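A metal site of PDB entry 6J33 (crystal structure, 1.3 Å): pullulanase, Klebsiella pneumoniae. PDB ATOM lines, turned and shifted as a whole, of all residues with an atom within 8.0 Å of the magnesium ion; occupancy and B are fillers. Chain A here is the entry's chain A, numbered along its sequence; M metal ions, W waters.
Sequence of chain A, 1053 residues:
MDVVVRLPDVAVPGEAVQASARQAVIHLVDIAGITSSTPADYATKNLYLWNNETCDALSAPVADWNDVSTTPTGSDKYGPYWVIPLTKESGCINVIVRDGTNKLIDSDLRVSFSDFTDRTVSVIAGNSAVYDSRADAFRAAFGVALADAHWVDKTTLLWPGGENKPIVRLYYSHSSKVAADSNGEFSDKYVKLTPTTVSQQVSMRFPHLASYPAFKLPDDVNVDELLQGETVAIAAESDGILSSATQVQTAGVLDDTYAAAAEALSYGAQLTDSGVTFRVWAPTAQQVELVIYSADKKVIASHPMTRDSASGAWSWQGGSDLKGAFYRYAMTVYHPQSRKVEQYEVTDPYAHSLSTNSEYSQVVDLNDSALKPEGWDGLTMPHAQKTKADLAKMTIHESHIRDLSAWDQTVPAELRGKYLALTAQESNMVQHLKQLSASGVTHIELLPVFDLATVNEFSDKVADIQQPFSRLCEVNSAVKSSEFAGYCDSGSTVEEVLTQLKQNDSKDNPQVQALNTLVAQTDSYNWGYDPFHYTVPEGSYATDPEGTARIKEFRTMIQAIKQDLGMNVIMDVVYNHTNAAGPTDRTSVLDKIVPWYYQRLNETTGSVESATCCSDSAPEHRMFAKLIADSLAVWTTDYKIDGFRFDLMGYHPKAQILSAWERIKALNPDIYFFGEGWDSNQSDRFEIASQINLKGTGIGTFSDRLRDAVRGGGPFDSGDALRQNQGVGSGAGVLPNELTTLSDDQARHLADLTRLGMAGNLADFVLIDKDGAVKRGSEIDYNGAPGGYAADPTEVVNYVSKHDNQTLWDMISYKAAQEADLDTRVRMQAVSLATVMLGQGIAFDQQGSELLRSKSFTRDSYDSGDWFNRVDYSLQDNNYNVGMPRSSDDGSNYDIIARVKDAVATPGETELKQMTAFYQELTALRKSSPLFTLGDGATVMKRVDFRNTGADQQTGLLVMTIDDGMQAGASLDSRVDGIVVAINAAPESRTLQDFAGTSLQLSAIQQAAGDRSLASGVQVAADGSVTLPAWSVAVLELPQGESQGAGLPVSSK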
ATOM      1  N   SER A 929      13.845  27.857 -21.661  1.00  0.00           N
ATOM      2  CA  SER A 929      14.813  28.344 -20.694  1.00  0.00           C
ATOM      3  C   SER A 929      14.210  29.545 -19.980  1.00  0.00           C
ATOM      4  O   SER A 929      13.556  30.370 -20.632  1.00  0.00           O
ATOM      5  CB  SER A 929      16.103  28.782 -21.379  1.00  0.00           C
ATOM      6  OG  SER A 929      16.998  29.345 -20.435  1.00  0.00           O
ATOM      7  N   LEU A 931      15.864  31.973 -19.342  1.00  0.00           N
ATOM      8  CA  LEU A 931      16.641  33.110 -19.827  1.00  0.00           C
ATOM      9  C   LEU A 931      15.904  33.934 -20.875  1.00  0.00           C
ATOM     10  O   LEU A 931      16.236  35.104 -21.052  1.00  0.00           O
ATOM     11  CB  LEU A 931      17.970  32.612 -20.400  1.00  0.00           C
ATOM     12  CG  LEU A 931      18.927  32.007 -19.359  1.00  0.00           C
ATOM     13  CD1 LEU A 931      20.111  31.359 -20.052  1.00  0.00           C
ATOM     14  CD2 LEU A 931      19.394  33.080 -18.401  1.00  0.00           C
ATOM     15  N   ARG A 943      22.127  40.958 -18.427  1.00  0.00           N
ATOM     16  CA  ARG A 943      22.338  39.726 -19.130  1.00  0.00           C
ATOM     17  C   ARG A 943      22.208  39.700 -20.651  1.00  0.00           C
ATOM     18  O   ARG A 943      22.788  38.860 -21.269  1.00  0.00           O
ATOM     19  CB  ARG A 943      21.387  38.669 -18.576  1.00  0.00           C
ATOM     20  CG  ARG A 943      21.589  38.314 -17.115  1.00  0.00           C
ATOM     21  CD  ARG A 943      20.529  37.387 -16.579  1.00  0.00           C
ATOM     22  NE  ARG A 943      20.749  37.066 -15.177  1.00  0.00           N
ATOM     23  CZ  ARG A 943      21.194  35.910 -14.727  1.00  0.00           C
ATOM     24  NH1 ARG A 943      21.562  34.961 -15.535  1.00  0.00           N
ATOM     25  NH2 ARG A 943      21.320  35.730 -13.447  1.00  0.00           N
ATOM     26  N   ASP A 963      23.179  36.057 -21.002  1.00  0.00           N
ATOM     27  CA  ASP A 963      24.215  35.542 -20.118  1.00  0.00           C
ATOM     28  C   ASP A 963      23.610  34.772 -18.946  1.00  0.00           C
ATOM     29  O   ASP A 963      22.670  35.232 -18.299  1.00  0.00           O
ATOM     30  CB  ASP A 963      25.058  36.699 -19.602  1.00  0.00           C
ATOM     31  CG  ASP A 963      26.316  36.245 -18.873  1.00  0.00           C
ATOM     32  OD1 ASP A 963      26.748  35.079 -19.064  1.00  0.00           O
ATOM     33  OD2 ASP A 963      26.869  37.063 -18.113  1.00  0.00           O
ATOM     34  N   ASP A 964      24.170  33.584 -18.680  1.00  0.00           N
ATOM     35  CA  ASP A 964      23.945  32.895 -17.423  1.00  0.00           C
ATOM     36  C   ASP A 964      25.237  32.650 -16.657  1.00  0.00           C
ATOM     37  O   ASP A 964      25.257  31.853 -15.707  1.00  0.00           O
ATOM     38  CB  ASP A 964      23.182  31.577 -17.633  1.00  0.00           C
ATOM     39  CG  ASP A 964      22.312  31.210 -16.429  1.00  0.00           C
ATOM     40  OD1 ASP A 964      21.781  32.118 -15.758  1.00  0.00           O
ATOM     41  OD2 ASP A 964      22.173  29.992 -16.175  1.00  0.00           O
ATOM     42  N   GLY A 965      26.331  33.319 -17.041  1.00  0.00           N
ATOM     43  CA  GLY A 965      27.615  33.092 -16.429  1.00  0.00           C
ATOM     44  C   GLY A 965      27.828  33.882 -15.144  1.00  0.00           C
ATOM     45  O   GLY A 965      26.963  34.624 -14.676  1.00  0.00           O
ATOM     46  N   ALA A 970      23.561  34.797 -10.340  1.00  0.00           N
ATOM     47  CA  ALA A 970      23.280  33.382 -10.182  1.00  0.00           C
ATOM     48  C   ALA A 970      22.969  32.750 -11.529  1.00  0.00           C
ATOM     49  O   ALA A 970      22.529  33.419 -12.475  1.00  0.00           O
ATOM     50  CB  ALA A 970      22.094  33.176  -9.239  1.00  0.00           C
ATOM     51  N   SER A 971      23.229  31.452 -11.632  1.00  0.00           N
ATOM     52  CA  SER A 971      22.738  30.684 -12.759  1.00  0.00           C
ATOM     53  C   SER A 971      21.233  30.535 -12.617  1.00  0.00           C
ATOM     54  O   SER A 971      20.752  29.995 -11.623  1.00  0.00           O
ATOM     55  CB  SER A 971      23.400  29.303 -12.768  1.00  0.00           C
ATOM     56  OG  SER A 971      22.802  28.456 -13.733  1.00  0.00           O
ATOM     57  N   LEU A 972      20.491  31.043 -13.604  1.00  0.00           N
ATOM     58  CA  LEU A 972      19.045  30.878 -13.624  1.00  0.00           C
ATOM     59  C   LEU A 972      18.614  29.648 -14.406  1.00  0.00           C
ATOM     60  O   LEU A 972      17.444  29.250 -14.307  1.00  0.00           O
ATOM     61  CB  LEU A 972      18.372  32.116 -14.218  1.00  0.00           C
ATOM     62  CG  LEU A 972      18.699  33.430 -13.539  1.00  0.00           C
ATOM     63  CD1 LEU A 972      18.123  34.590 -14.332  1.00  0.00           C
ATOM     64  CD2 LEU A 972      18.159  33.431 -12.115  1.00  0.00           C
ATOM     65  N   ASP A 973      19.513  29.040 -15.171  1.00  0.00           N
ATOM     66  CA  ASP A 973      19.245  27.829 -15.929  1.00  0.00           C
ATOM     67  C   ASP A 973      20.392  26.866 -15.657  1.00  0.00           C
ATOM     68  O   ASP A 973      21.536  27.135 -16.024  1.00  0.00           O
ATOM     69  CB  ASP A 973      19.154  28.133 -17.427  1.00  0.00           C
ATOM     70  CG  ASP A 973      18.692  26.932 -18.252  1.00  0.00           C
ATOM     71  OD1 ASP A 973      19.021  25.780 -17.890  1.00  0.00           O
ATOM     72  OD2 ASP A 973      17.988  27.144 -19.260  1.00  0.00           O
ATOM     73  N   SER A 974      20.076  25.733 -15.032  1.00  0.00           N
ATOM     74  CA  SER A 974      21.111  24.785 -14.635  1.00  0.00           C
ATOM     75  C   SER A 974      21.725  24.051 -15.823  1.00  0.00           C
ATOM     76  O   SER A 974      22.781  23.429 -15.668  1.00  0.00           O
ATOM     77  CB  SER A 974      20.535  23.764 -13.647  1.00  0.00           C
ATOM     78  OG  SER A 974      19.509  23.008 -14.249  1.00  0.00           O
ATOM     79  N   ARG A 975      21.090  24.091 -16.995  1.00  0.00           N
ATOM     80  CA  ARG A 975      21.608  23.382 -18.163  1.00  0.00           C
ATOM     81  C   ARG A 975      22.613  24.191 -18.962  1.00  0.00           C
ATOM     82  O   ARG A 975      23.465  23.608 -19.635  1.00  0.00           O
ATOM     83  CB  ARG A 975      20.465  23.003 -19.112  1.00  0.00           C
ATOM     84  CG  ARG A 975      19.322  22.235 -18.492  1.00  0.00           C
ATOM     85  CD  ARG A 975      18.136  22.205 -19.456  1.00  0.00           C
ATOM     86  NE  ARG A 975      17.707  23.555 -19.816  1.00  0.00           N
ATOM     87  CZ  ARG A 975      17.890  24.118 -21.003  1.00  0.00           C
ATOM     88  NH1 ARG A 975      17.453  25.356 -21.210  1.00  0.00           N
ATOM     89  NH2 ARG A 975      18.492  23.465 -21.984  1.00  0.00           N
ATOM     90  N   VAL A 976      22.524  25.513 -18.924  1.00  0.00           N
ATOM     91  CA  VAL A 976      23.314  26.368 -19.806  1.00  0.00           C
ATOM     92  C   VAL A 976      23.975  27.505 -19.029  1.00  0.00           C
ATOM     93  O   VAL A 976      23.465  27.973 -18.008  1.00  0.00           O
ATOM     94  CB  VAL A 976      22.478  26.950 -20.971  1.00  0.00           C
ATOM     95  CG1 VAL A 976      21.828  25.832 -21.789  1.00  0.00           C
ATOM     96  CG2 VAL A 976      21.432  27.929 -20.467  1.00  0.00           C
ATOM     97  N   ASP A 977      25.123  27.949 -19.546  1.00  0.00           N
ATOM     98  CA  ASP A 977      25.785  29.166 -19.105  1.00  0.00           C
ATOM     99  C   ASP A 977      25.431  30.369 -19.972  1.00  0.00           C
ATOM    100  O   ASP A 977      25.882  31.488 -19.681  1.00  0.00           O
ATOM    101  CB  ASP A 977      27.300  28.977 -19.087  1.00  0.00           C
ATOM    102  CG  ASP A 977      27.764  28.031 -17.980  1.00  0.00           C
ATOM    103  OD1 ASP A 977      27.248  28.135 -16.851  1.00  0.00           O
ATOM    104  OD2 ASP A 977      28.655  27.212 -18.250  1.00  0.00           O
ATOM    105  N   GLY A 978      24.673  30.168 -21.039  1.00  0.00           N
ATOM    106  CA  GLY A 978      24.267  31.272 -21.884  1.00  0.00           C
ATOM    107  C   GLY A 978      23.541  30.756 -23.105  1.00  0.00           C
ATOM    108  O   GLY A 978      23.623  29.567 -23.438  1.00  0.00           O
ATOM    109  N   LEU A1038      25.322  27.388 -24.509  1.00  0.00           N
ATOM    110  CA  LEU A1038      26.590  27.029 -23.885  1.00  0.00           C
ATOM    111  C   LEU A1038      26.257  26.037 -22.769  1.00  0.00           C
ATOM    112  O   LEU A1038      25.701  26.442 -21.749  1.00  0.00           O
ATOM    113  CB  LEU A1038      27.262  28.259 -23.290  1.00  0.00           C
ATOM    114  CG  LEU A1038      27.925  29.296 -24.189  1.00  0.00           C
ATOM    115  CD1 LEU A1038      28.481  30.422 -23.336  1.00  0.00           C
ATOM    116  CD2 LEU A1038      29.046  28.662 -25.009  1.00  0.00           C
ATOM    117  N   PRO A1039      26.576  24.756 -22.926  1.00  0.00           N
ATOM    118  CA  PRO A1039      26.177  23.778 -21.903  1.00  0.00           C
ATOM    119  C   PRO A1039      26.899  24.038 -20.595  1.00  0.00           C
ATOM    120  O   PRO A1039      28.087  24.388 -20.577  1.00  0.00           O
ATOM    121  CB  PRO A1039      26.602  22.429 -22.512  1.00  0.00           C
ATOM    122  CG  PRO A1039      26.912  22.708 -23.932  1.00  0.00           C
ATOM    123  CD  PRO A1039      27.322  24.130 -24.032  1.00  0.00           C
ATOM    124  N   GLN A1040      26.181  23.872 -19.493  1.00  0.00           N
ATOM    125  CA  GLN A1040      26.728  24.142 -18.182  1.00  0.00           C
ATOM    126  C   GLN A1040      27.386  22.879 -17.642  1.00  0.00           C
ATOM    127  O   GLN A1040      26.783  21.797 -17.653  1.00  0.00           O
ATOM    128  CB  GLN A1040      25.635  24.630 -17.219  1.00  0.00           C
ATOM    129  CG  GLN A1040      26.162  25.116 -15.880  1.00  0.00           C
ATOM    130  CD  GLN A1040      25.115  25.868 -15.083  1.00  0.00           C
ATOM    131  OE1 GLN A1040      24.267  26.570 -15.654  1.00  0.00           O
ATOM    132  NE2 GLN A1040      25.152  25.741 -13.762  1.00  0.00           N
ATOM    133  N   GLY A1041      28.639  23.017 -17.203  1.00  0.00           N
ATOM    134  CA  GLY A1041      29.393  21.893 -16.687  1.00  0.00           C
ATOM    135  C   GLY A1041      29.171  21.622 -15.208  1.00  0.00           C
ATOM    136  O   GLY A1041      28.057  21.766 -14.710  1.00  0.00           O
ATOM    137  N   SER A1043      30.214  23.284 -12.630  1.00  0.00           N
ATOM    138  CA  SER A1043      29.874  24.520 -11.947  1.00  0.00           C
ATOM    139  C   SER A1043      29.551  25.583 -12.976  1.00  0.00           C
ATOM    140  O   SER A1043      29.829  25.426 -14.173  1.00  0.00           O
ATOM    141  CB  SER A1043      31.007  24.986 -11.020  1.00  0.00           C
ATOM    142  OG  SER A1043      31.270  24.033 -10.006  1.00  0.00           O
ATOM    143  N   GLN A1044      28.938  26.680 -12.509  1.00  0.00           N
ATOM    144  CA  GLN A1044      28.575  27.777 -13.386  1.00  0.00           C
ATOM    145  C   GLN A1044      29.811  28.309 -14.104  1.00  0.00           C
ATOM    146  O   GLN A1044      30.875  28.488 -13.484  1.00  0.00           O
ATOM    147  CB  GLN A1044      27.940  28.901 -12.576  1.00  0.00           C
ATOM    148  CG  GLN A1044      27.646  30.182 -13.353  1.00  0.00           C
ATOM    149  CD  GLN A1044      27.126  31.302 -12.456  1.00  0.00           C
ATOM    150  OE1 GLN A1044      27.549  31.430 -11.306  1.00  0.00           O
ATOM    151  NE2 GLN A1044      26.215  32.111 -12.976  1.00  0.00           N
ATOM    152  N   GLY A1045      29.682  28.553 -15.413  1.00  0.00           N
ATOM    153  CA  GLY A1045      30.792  28.914 -16.250  1.00  0.00           C
ATOM    154  C   GLY A1045      30.875  30.401 -16.547  1.00  0.00           C
ATOM    155  O   GLY A1045      30.201  31.239 -15.933  1.00  0.00           O
HETATM  156 MG    MG M   1      23.235  28.217 -15.900  1.00  0.00          MG
HETATM  157  O   HOH W   1      25.079  29.214 -15.716  1.00  0.00           O
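The backbone carbonyl oxygen (O) of Asp 964 sits at hydrogen-bond distance from the side-chain amide nitrogen (NE2) of Gln 1044 (2.9 Å).
The backbone NH of Leu 972 sits at hydrogen-bond distance from the side-chain carboxylate of Asp 964, at 2.7 Å.
The backbone NH of Gln 1040 is in hydrogen-bond range of the backbone carbonyl oxygen of Arg 975 (2.7 Å).
The side-chain carboxylate (OD1) of Asp 964 is in salt-bridge range of the guanidinium group (NH1) of Arg 943, 2.9 Å away.
N of Ser 971 sits close to NE2 of Gln 1044 (3.3 Å).
The guanidinium group (NH1) of Arg 975 lies within salt-bridge range of the side-chain carboxylate (OD2) of Asp 973, 2.7 Å away.
OD2 of Asp 973 sits at hydrogen-bond distance from OG of Ser 929 (2.7 Å).
OE1 of Gln 1040 lies close to O of Ser 974.
Of the 22 residues printed, 5 come within 4 Å of the magnesium ion.
The magnesium ion is bound by OE1 of Gln 1040 (2.0 Å), O of Asp 973 (2.0 Å), OD2 of Asp 964 (2.1 Å), water W1 (2.1 Å), O of Val 976 (2.1 Å) and OG of Ser 971 (2.2 Å).
The magnesium ion has six donor atoms within binding distance.
Water W1 lies within hydrogen-bond range of O of Asp 964 (2.6 Å) and OD1 of Asp 977 (2.7 Å).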
